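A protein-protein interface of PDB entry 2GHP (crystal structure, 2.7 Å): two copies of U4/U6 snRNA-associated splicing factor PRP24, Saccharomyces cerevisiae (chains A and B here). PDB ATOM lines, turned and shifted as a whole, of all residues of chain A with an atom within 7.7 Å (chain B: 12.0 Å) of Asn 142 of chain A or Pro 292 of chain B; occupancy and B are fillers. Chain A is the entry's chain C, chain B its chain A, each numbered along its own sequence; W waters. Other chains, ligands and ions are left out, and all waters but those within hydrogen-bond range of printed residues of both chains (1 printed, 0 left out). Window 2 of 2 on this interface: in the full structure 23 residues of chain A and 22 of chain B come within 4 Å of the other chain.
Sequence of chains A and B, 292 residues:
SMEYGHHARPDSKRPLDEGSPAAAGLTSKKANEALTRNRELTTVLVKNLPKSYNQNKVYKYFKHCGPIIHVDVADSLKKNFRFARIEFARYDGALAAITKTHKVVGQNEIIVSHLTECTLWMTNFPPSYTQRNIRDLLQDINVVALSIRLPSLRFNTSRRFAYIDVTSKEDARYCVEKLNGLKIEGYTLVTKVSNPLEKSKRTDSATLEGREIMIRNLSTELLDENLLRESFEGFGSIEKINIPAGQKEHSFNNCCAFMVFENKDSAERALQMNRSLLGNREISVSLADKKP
The side-chain carboxylate (OE2) of Glu 209 of chain B sits at hydrogen-bond distance from the backbone NH (N) of Asp 171 of chain A. The backbone carbonyl oxygen (O) of Ala 288 of chain B is in hydrogen-bond range of the side-chain hydroxyl (OH) of Tyr 174 of chain A, 3.0 Å away. The side-chain amide nitrogen (ND2) of Asn 142 of chain A is in hydrogen-bond range of the backbone carbonyl oxygen (O) of Lys 290 of chain B (2.9 Å). NZ of Lys 290 of chain B lies within salt-bridge range of OD1 of Asp 171 of chain A (2.9 Å). The side-chain hydroxyl of Tyr 174 of chain A sits at hydrogen-bond distance from the backbone NH of Lys 290 of chain B (3.3 Å). The chain-end carboxylate (OXT) of Pro 292 of chain B lies within salt-bridge range of the side-chain amino group (NZ) of Lys 78 of chain A, at 3.3 Å.
OE1 of Glu 209 of chain B lies within salt-bridge range of NZ of Lys 290 of chain B (2.9 Å). The backbone NH of Ala 288 of chain B sits at hydrogen-bond distance from the backbone carbonyl oxygen of Glu 212 of chain B (3.0 Å). OG of Ser 76 of chain A lies close to N of Lys 78 of chain A, at 3.5 Å.
Ile 141 of chain A touches Lys 290 of chain B (O to CG, 3.5 Å). Asn 142 of chain A touches Pro 292 of chain B. Tyr 174 of chain A touches Glu 209 of chain B (CB to OE2, 3.5 Å). Leu 287 of chain B touches Tyr 174 of chain A. OH of Tyr 174 of chain A touches CA of Asp 289 of chain B (3.2 Å).
Of the printed residues of chain B, Asn 142 of chain A touches Lys 290 (2.9 Å) and Pro 292 (3.7 Å). Pro 292 of chain B touches just these residues of chain A: Lys 78 (3.3 Å) and Asn 142 (3.7 Å). Leu 138 of chain A touches none of the printed residues of chain B. No residue of chain B comes within 4 Å of Asp 140 of chain A. Of the printed residues of chain B, Ile 141 of chain A touches Lys 290. No residue of chain B comes within 4 Å of Val 144 of chain A. Of the printed residues of chain B, Asp 171 of chain A touches Glu 209 and Lys 290. Printed residues of chain A within 4 Å of Lys 290 of chain B: Ile 141 (3.5 Å), Asn 142 (2.9 Å), Asp 171 (2.9 Å) and Tyr 174 (3.3 Å). Of the printed residues of chain A, Asp 289 of chain B touches Tyr 174. The nearest residue of chain A that does not touch Pro 292 of chain B is Leu 77 of chain A (4.04 Å). The nearest printed residue of chain A that does not touch Asp 289 of chain B is Asn 142 of chain A (5.3 Å).
Hydrophobic or aromatic side chains of chain A within 4 Å of the printed part of chain B: Tyr 174. Printed residues of chain B that touch a printed residue of chain A: Glu 209, Leu 287, Ala 288, Asp 289, Lys 290 and Pro 292. Hydrophobic or aromatic side chains of chain B within 4 Å of the printed part of chain A: Leu 287. Among the printed residues, 11 pairs touch across the chains.
No position is printed for both chains.
Water W1 lies within hydrogen-bond range of OD2 of Asp 171 of chain A (2.9 Å), N of Val 144 of chain A (3.2 Å), NZ of Lys 290 of chain B (3.2 Å) and O of Asn 142 of chain A (3.5 Å).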
ATOM      1  N   SER A  76       7.099 -15.664  15.845  1.00  0.00           N
ATOM      2  CA  SER A  76       8.524 -15.960  15.765  1.00  0.00           C
ATOM      3  C   SER A  76       9.270 -14.641  15.612  1.00  0.00           C
ATOM      4  O   SER A  76       8.680 -13.644  15.188  1.00  0.00           O
ATOM      5  CB  SER A  76       8.837 -16.942  14.614  1.00  0.00           C
ATOM      6  OG  SER A  76       9.194 -16.334  13.368  1.00  0.00           O
ATOM      7  N   LEU A  77      10.546 -14.627  15.989  1.00  0.00           N
ATOM      8  CA  LEU A  77      11.400 -13.441  15.842  1.00  0.00           C
ATOM      9  C   LEU A  77      11.240 -12.747  14.495  1.00  0.00           C
ATOM     10  O   LEU A  77      11.082 -11.531  14.434  1.00  0.00           O
ATOM     11  CB  LEU A  77      12.870 -13.837  16.015  1.00  0.00           C
ATOM     12  CG  LEU A  77      13.645 -13.496  17.288  1.00  0.00           C
ATOM     13  CD1 LEU A  77      12.732 -13.298  18.497  1.00  0.00           C
ATOM     14  CD2 LEU A  77      14.718 -14.569  17.555  1.00  0.00           C
ATOM     15  N   LYS A  78      11.277 -13.540  13.423  1.00  0.00           N
ATOM     16  CA  LYS A  78      11.236 -13.041  12.063  1.00  0.00           C
ATOM     17  C   LYS A  78       9.809 -13.154  11.525  1.00  0.00           C
ATOM     18  O   LYS A  78       9.563 -13.068  10.319  1.00  0.00           O
ATOM     19  CB  LYS A  78      12.211 -13.857  11.234  1.00  0.00           C
ATOM     20  CG  LYS A  78      13.491 -14.224  12.003  1.00  0.00           C
ATOM     21  CD  LYS A  78      14.127 -15.563  11.531  1.00  0.00           C
ATOM     22  CE  LYS A  78      14.947 -15.413  10.244  1.00  0.00           C
ATOM     23  NZ  LYS A  78      15.938 -14.311  10.369  1.00  0.00           N
ATOM     24  N   ARG A 135       7.382  -6.980  26.800  1.00  0.00           N
ATOM     25  CA  ARG A 135       7.633  -7.640  25.519  1.00  0.00           C
ATOM     26  C   ARG A 135       8.672  -6.902  24.670  1.00  0.00           C
ATOM     27  O   ARG A 135       9.443  -7.544  23.960  1.00  0.00           O
ATOM     28  CB  ARG A 135       6.334  -7.860  24.736  1.00  0.00           C
ATOM     29  CG  ARG A 135       6.483  -8.787  23.528  1.00  0.00           C
ATOM     30  CD  ARG A 135       5.168  -8.939  22.737  1.00  0.00           C
ATOM     31  NE  ARG A 135       4.170  -9.733  23.458  1.00  0.00           N
ATOM     32  CZ  ARG A 135       4.210 -11.063  23.603  1.00  0.00           C
ATOM     33  NH1 ARG A 135       5.202 -11.780  23.077  1.00  0.00           N
ATOM     34  NH2 ARG A 135       3.258 -11.687  24.286  1.00  0.00           N
ATOM     35  N   ASP A 136       8.689  -5.567  24.754  1.00  0.00           N
ATOM     36  CA  ASP A 136       9.657  -4.729  24.016  1.00  0.00           C
ATOM     37  C   ASP A 136      11.067  -5.002  24.493  1.00  0.00           C
ATOM     38  O   ASP A 136      12.013  -5.081  23.699  1.00  0.00           O
ATOM     39  CB  ASP A 136       9.367  -3.252  24.246  1.00  0.00           C
ATOM     40  CG  ASP A 136       8.138  -2.780  23.521  1.00  0.00           C
ATOM     41  OD1 ASP A 136       7.645  -3.520  22.639  1.00  0.00           O
ATOM     42  OD2 ASP A 136       7.669  -1.659  23.834  1.00  0.00           O
ATOM     43  N   LEU A 137      11.191  -5.131  25.812  1.00  0.00           N
ATOM     44  CA  LEU A 137      12.450  -5.422  26.428  1.00  0.00           C
ATOM     45  C   LEU A 137      12.990  -6.701  25.828  1.00  0.00           C
ATOM     46  O   LEU A 137      14.147  -6.739  25.404  1.00  0.00           O
ATOM     47  CB  LEU A 137      12.295  -5.564  27.936  1.00  0.00           C
ATOM     48  CG  LEU A 137      12.794  -4.441  28.826  1.00  0.00           C
ATOM     49  CD1 LEU A 137      12.732  -4.880  30.257  1.00  0.00           C
ATOM     50  CD2 LEU A 137      14.219  -4.141  28.459  1.00  0.00           C
ATOM     51  N   LEU A 138      12.158  -7.739  25.757  1.00  0.00           N
ATOM     52  CA  LEU A 138      12.657  -9.019  25.307  1.00  0.00           C
ATOM     53  C   LEU A 138      12.977  -8.978  23.824  1.00  0.00           C
ATOM     54  O   LEU A 138      13.897  -9.622  23.359  1.00  0.00           O
ATOM     55  CB  LEU A 138      11.696 -10.146  25.668  1.00  0.00           C
ATOM     56  CG  LEU A 138      11.943 -10.896  26.972  1.00  0.00           C
ATOM     57  CD1 LEU A 138      12.257  -9.965  28.113  1.00  0.00           C
ATOM     58  CD2 LEU A 138      10.719 -11.698  27.293  1.00  0.00           C
ATOM     59  N   GLN A 139      12.227  -8.189  23.087  1.00  0.00           N
ATOM     60  CA  GLN A 139      12.493  -8.017  21.674  1.00  0.00           C
ATOM     61  C   GLN A 139      13.793  -7.257  21.474  1.00  0.00           C
ATOM     62  O   GLN A 139      14.481  -7.494  20.484  1.00  0.00           O
ATOM     63  CB  GLN A 139      11.347  -7.268  20.995  1.00  0.00           C
ATOM     64  CG  GLN A 139      11.331  -7.380  19.485  1.00  0.00           C
ATOM     65  CD  GLN A 139      10.604  -6.217  18.834  1.00  0.00           C
ATOM     66  OE1 GLN A 139      10.477  -5.134  19.417  1.00  0.00           O
ATOM     67  NE2 GLN A 139      10.124  -6.430  17.618  1.00  0.00           N
ATOM     68  N   ASP A 140      14.128  -6.345  22.392  1.00  0.00           N
ATOM     69  CA  ASP A 140      15.402  -5.622  22.288  1.00  0.00           C
ATOM     70  C   ASP A 140      16.585  -6.593  22.349  1.00  0.00           C
ATOM     71  O   ASP A 140      17.642  -6.305  21.803  1.00  0.00           O
ATOM     72  CB  ASP A 140      15.570  -4.541  23.364  1.00  0.00           C
ATOM     73  CG  ASP A 140      14.594  -3.385  23.214  1.00  0.00           C
ATOM     74  OD1 ASP A 140      14.082  -3.122  22.103  1.00  0.00           O
ATOM     75  OD2 ASP A 140      14.342  -2.712  24.232  1.00  0.00           O
ATOM     76  N   ILE A 141      16.413  -7.739  23.006  1.00  0.00           N
ATOM     77  CA  ILE A 141      17.481  -8.738  23.076  1.00  0.00           C
ATOM     78  C   ILE A 141      17.171  -9.977  22.251  1.00  0.00           C
ATOM     79  O   ILE A 141      17.830 -11.011  22.414  1.00  0.00           O
ATOM     80  CB  ILE A 141      17.799  -9.140  24.523  1.00  0.00           C
ATOM     81  CG1 ILE A 141      16.557  -9.683  25.232  1.00  0.00           C
ATOM     82  CG2 ILE A 141      18.350  -7.957  25.257  1.00  0.00           C
ATOM     83  CD1 ILE A 141      16.863 -10.610  26.341  1.00  0.00           C
ATOM     84  N   ASN A 142      16.179  -9.850  21.364  1.00  0.00           N
ATOM     85  CA  ASN A 142      15.734 -10.915  20.439  1.00  0.00           C
ATOM     86  C   ASN A 142      15.255 -12.201  21.085  1.00  0.00           C
ATOM     87  O   ASN A 142      15.715 -13.291  20.756  1.00  0.00           O
ATOM     88  CB  ASN A 142      16.802 -11.209  19.391  1.00  0.00           C
ATOM     89  CG  ASN A 142      16.842 -10.166  18.310  1.00  0.00           C
ATOM     90  OD1 ASN A 142      15.798  -9.713  17.827  1.00  0.00           O
ATOM     91  ND2 ASN A 142      18.049  -9.772  17.913  1.00  0.00           N
ATOM     92  N   VAL A 143      14.327 -12.055  22.017  1.00  0.00           N
ATOM     93  CA  VAL A 143      13.762 -13.195  22.716  1.00  0.00           C
ATOM     94  C   VAL A 143      12.261 -13.107  22.604  1.00  0.00           C
ATOM     95  O   VAL A 143      11.687 -12.056  22.887  1.00  0.00           O
ATOM     96  CB  VAL A 143      14.186 -13.243  24.198  1.00  0.00           C
ATOM     97  CG1 VAL A 143      13.365 -14.264  24.983  1.00  0.00           C
ATOM     98  CG2 VAL A 143      15.646 -13.580  24.296  1.00  0.00           C
ATOM     99  N   VAL A 144      11.635 -14.201  22.166  1.00  0.00           N
ATOM    100  CA  VAL A 144      10.188 -14.300  22.069  1.00  0.00           C
ATOM    101  C   VAL A 144       9.580 -14.452  23.446  1.00  0.00           C
ATOM    102  O   VAL A 144       9.994 -15.309  24.227  1.00  0.00           O
ATOM    103  CB  VAL A 144       9.788 -15.505  21.246  1.00  0.00           C
ATOM    104  CG1 VAL A 144       8.299 -15.766  21.379  1.00  0.00           C
ATOM    105  CG2 VAL A 144      10.176 -15.279  19.786  1.00  0.00           C
ATOM    106  N   ALA A 145       8.608 -13.604  23.752  1.00  0.00           N
ATOM    107  CA  ALA A 145       7.815 -13.794  24.955  1.00  0.00           C
ATOM    108  C   ALA A 145       6.618 -14.679  24.626  1.00  0.00           C
ATOM    109  O   ALA A 145       5.687 -14.283  23.924  1.00  0.00           O
ATOM    110  CB  ALA A 145       7.382 -12.468  25.558  1.00  0.00           C
ATOM    111  N   ASP A 171      16.965 -19.310  26.209  1.00  0.00           N
ATOM    112  CA  ASP A 171      16.356 -17.989  26.239  1.00  0.00           C
ATOM    113  C   ASP A 171      16.104 -17.506  27.663  1.00  0.00           C
ATOM    114  O   ASP A 171      16.429 -16.369  27.988  1.00  0.00           O
ATOM    115  CB  ASP A 171      15.093 -17.930  25.400  1.00  0.00           C
ATOM    116  CG  ASP A 171      15.383 -17.556  23.952  1.00  0.00           C
ATOM    117  OD1 ASP A 171      16.546 -17.211  23.660  1.00  0.00           O
ATOM    118  OD2 ASP A 171      14.463 -17.588  23.105  1.00  0.00           O
ATOM    119  N   TYR A 174      19.655 -16.588  29.031  1.00  0.00           N
ATOM    120  CA  TYR A 174      20.192 -15.474  28.269  1.00  0.00           C
ATOM    121  C   TYR A 174      19.473 -14.202  28.667  1.00  0.00           C
ATOM    122  O   TYR A 174      20.075 -13.167  28.949  1.00  0.00           O
ATOM    123  CB  TYR A 174      19.965 -15.730  26.795  1.00  0.00           C
ATOM    124  CG  TYR A 174      20.491 -14.644  25.891  1.00  0.00           C
ATOM    125  CD1 TYR A 174      21.862 -14.439  25.739  1.00  0.00           C
ATOM    126  CD2 TYR A 174      19.621 -13.844  25.165  1.00  0.00           C
ATOM    127  CE1 TYR A 174      22.345 -13.461  24.900  1.00  0.00           C
ATOM    128  CE2 TYR A 174      20.097 -12.859  24.321  1.00  0.00           C
ATOM    129  CZ  TYR A 174      21.456 -12.671  24.196  1.00  0.00           C
ATOM    130  OH  TYR A 174      21.934 -11.697  23.348  1.00  0.00           O
ATOM    131  N   THR B 207      22.168 -21.234  18.105  1.00  0.00           N
ATOM    132  CA  THR B 207      23.362 -22.071  18.249  1.00  0.00           C
ATOM    133  C   THR B 207      24.415 -21.268  18.967  1.00  0.00           C
ATOM    134  O   THR B 207      24.970 -21.719  19.988  1.00  0.00           O
ATOM    135  CB  THR B 207      24.041 -22.468  16.897  1.00  0.00           C
ATOM    136  OG1 THR B 207      23.074 -22.679  15.840  1.00  0.00           O
ATOM    137  CG2 THR B 207      24.944 -23.706  17.100  1.00  0.00           C
ATOM    138  N   LEU B 208      24.694 -20.082  18.413  1.00  0.00           N
ATOM    139  CA  LEU B 208      25.674 -19.142  18.966  1.00  0.00           C
ATOM    140  C   LEU B 208      25.265 -18.559  20.314  1.00  0.00           C
ATOM    141  O   LEU B 208      26.104 -18.042  21.046  1.00  0.00           O
ATOM    142  CB  LEU B 208      25.907 -17.988  17.985  1.00  0.00           C
ATOM    143  CG  LEU B 208      26.828 -18.304  16.814  1.00  0.00           C
ATOM    144  CD1 LEU B 208      26.951 -17.096  15.862  1.00  0.00           C
ATOM    145  CD2 LEU B 208      28.189 -18.774  17.369  1.00  0.00           C
ATOM    146  N   GLU B 209      23.973 -18.629  20.626  1.00  0.00           N
ATOM    147  CA  GLU B 209      23.419 -17.949  21.771  1.00  0.00           C
ATOM    148  C   GLU B 209      24.104 -18.416  23.065  1.00  0.00           C
ATOM    149  O   GLU B 209      24.068 -19.598  23.424  1.00  0.00           O
ATOM    150  CB  GLU B 209      21.904 -18.159  21.806  1.00  0.00           C
ATOM    151  CG  GLU B 209      21.199 -17.525  22.992  1.00  0.00           C
ATOM    152  CD  GLU B 209      19.693 -17.683  22.946  1.00  0.00           C
ATOM    153  OE1 GLU B 209      19.143 -17.844  21.862  1.00  0.00           O
ATOM    154  OE2 GLU B 209      19.037 -17.640  23.994  1.00  0.00           O
ATOM    155  N   GLY B 210      24.763 -17.483  23.741  1.00  0.00           N
ATOM    156  CA  GLY B 210      25.356 -17.744  25.037  1.00  0.00           C
ATOM    157  C   GLY B 210      26.724 -18.366  24.914  1.00  0.00           C
ATOM    158  O   GLY B 210      27.320 -18.745  25.931  1.00  0.00           O
ATOM    159  N   GLU B 212      28.886 -16.772  22.305  1.00  0.00           N
ATOM    160  CA  GLU B 212      29.627 -15.663  21.689  1.00  0.00           C
ATOM    161  C   GLU B 212      29.778 -14.480  22.641  1.00  0.00           C
ATOM    162  O   GLU B 212      28.826 -14.078  23.326  1.00  0.00           O
ATOM    163  CB  GLU B 212      28.971 -15.202  20.370  1.00  0.00           C
ATOM    164  CG  GLU B 212      29.953 -14.506  19.414  1.00  0.00           C
ATOM    165  CD  GLU B 212      29.283 -13.760  18.272  1.00  0.00           C
ATOM    166  OE1 GLU B 212      28.518 -14.380  17.496  1.00  0.00           O
ATOM    167  OE2 GLU B 212      29.537 -12.544  18.133  1.00  0.00           O
ATOM    168  N   PHE B 258      34.940 -10.156  18.236  1.00  0.00           N
ATOM    169  CA  PHE B 258      33.989 -11.165  18.669  1.00  0.00           C
ATOM    170  C   PHE B 258      34.669 -12.501  18.812  1.00  0.00           C
ATOM    171  O   PHE B 258      35.464 -12.893  17.962  1.00  0.00           O
ATOM    172  CB  PHE B 258      32.839 -11.298  17.678  1.00  0.00           C
ATOM    173  CG  PHE B 258      32.058 -10.033  17.474  1.00  0.00           C
ATOM    174  CD1 PHE B 258      31.047  -9.669  18.355  1.00  0.00           C
ATOM    175  CD2 PHE B 258      32.322  -9.210  16.387  1.00  0.00           C
ATOM    176  CE1 PHE B 258      30.334  -8.505  18.156  1.00  0.00           C
ATOM    177  CE2 PHE B 258      31.603  -8.043  16.185  1.00  0.00           C
ATOM    178  CZ  PHE B 258      30.614  -7.695  17.061  1.00  0.00           C
ATOM    179  N   LEU B 287      28.125 -10.816  26.640  1.00  0.00           N
ATOM    180  CA  LEU B 287      27.478 -11.717  25.707  1.00  0.00           C
ATOM    181  C   LEU B 287      27.022 -10.952  24.461  1.00  0.00           C
ATOM    182  O   LEU B 287      26.381  -9.898  24.568  1.00  0.00           O
ATOM    183  CB  LEU B 287      26.294 -12.413  26.373  1.00  0.00           C
ATOM    184  CG  LEU B 287      26.601 -13.556  27.335  1.00  0.00           C
ATOM    185  CD1 LEU B 287      25.306 -14.272  27.731  1.00  0.00           C
ATOM    186  CD2 LEU B 287      27.599 -14.559  26.758  1.00  0.00           C
ATOM    187  N   ALA B 288      27.363 -11.457  23.281  1.00  0.00           N
ATOM    188  CA  ALA B 288      26.921 -10.818  22.045  1.00  0.00           C
ATOM    189  C   ALA B 288      25.388 -10.892  21.958  1.00  0.00           C
ATOM    190  O   ALA B 288      24.789 -11.777  22.567  1.00  0.00           O
ATOM    191  CB  ALA B 288      27.560 -11.513  20.866  1.00  0.00           C
ATOM    192  N   ASP B 289      24.738  -9.969  21.248  1.00  0.00           N
ATOM    193  CA  ASP B 289      23.304 -10.126  20.986  1.00  0.00           C
ATOM    194  C   ASP B 289      23.135 -11.314  20.062  1.00  0.00           C
ATOM    195  O   ASP B 289      24.059 -11.661  19.329  1.00  0.00           O
ATOM    196  CB  ASP B 289      22.696  -8.907  20.302  1.00  0.00           C
ATOM    197  CG  ASP B 289      23.161  -7.611  20.893  1.00  0.00           C
ATOM    198  OD1 ASP B 289      23.415  -7.579  22.107  1.00  0.00           O
ATOM    199  OD2 ASP B 289      23.259  -6.613  20.140  1.00  0.00           O
ATOM    200  N   LYS B 290      21.965 -11.942  20.089  1.00  0.00           N
ATOM    201  CA  LYS B 290      21.647 -12.974  19.104  1.00  0.00           C
ATOM    202  C   LYS B 290      21.237 -12.297  17.813  1.00  0.00           C
ATOM    203  O   LYS B 290      20.542 -11.288  17.843  1.00  0.00           O
ATOM    204  CB  LYS B 290      20.585 -13.963  19.616  1.00  0.00           C
ATOM    205  CG  LYS B 290      19.534 -13.405  20.594  1.00  0.00           C
ATOM    206  CD  LYS B 290      18.751 -14.529  21.299  1.00  0.00           C
ATOM    207  CE  LYS B 290      17.971 -15.415  20.319  1.00  0.00           C
ATOM    208  NZ  LYS B 290      16.931 -16.270  20.965  1.00  0.00           N
ATOM    209  N   LYS B 291      21.704 -12.832  16.685  1.00  0.00           N
ATOM    210  CA  LYS B 291      21.531 -12.164  15.384  1.00  0.00           C
ATOM    211  C   LYS B 291      20.062 -12.195  14.973  1.00  0.00           C
ATOM    212  O   LYS B 291      19.434 -13.254  15.059  1.00  0.00           O
ATOM    213  CB  LYS B 291      22.414 -12.789  14.288  1.00  0.00           C
ATOM    214  CG  LYS B 291      23.839 -13.185  14.720  1.00  0.00           C
ATOM    215  CD  LYS B 291      24.806 -12.009  14.908  1.00  0.00           C
ATOM    216  CE  LYS B 291      25.965 -12.426  15.840  1.00  0.00           C
ATOM    217  NZ  LYS B 291      27.018 -11.371  16.014  1.00  0.00           N
ATOM    218  N   PRO B 292      19.514 -11.037  14.519  1.00  0.00           N
ATOM    219  CA  PRO B 292      18.060 -10.873  14.330  1.00  0.00           C
ATOM    220  C   PRO B 292      17.384 -12.124  13.763  1.00  0.00           C
ATOM    221  O   PRO B 292      16.595 -12.769  14.459  1.00  0.00           O
ATOM    222  CB  PRO B 292      17.963  -9.688  13.357  1.00  0.00           C
ATOM    223  CG  PRO B 292      19.157  -8.839  13.701  1.00  0.00           C
ATOM    224  CD  PRO B 292      20.250  -9.809  14.132  1.00  0.00           C
ATOM    225  OXT PRO B 292      17.626 -12.540  12.627  1.00  0.00           O
HETATM  226  O   HOH W   1      13.735 -16.139  20.746  1.00  0.00           O
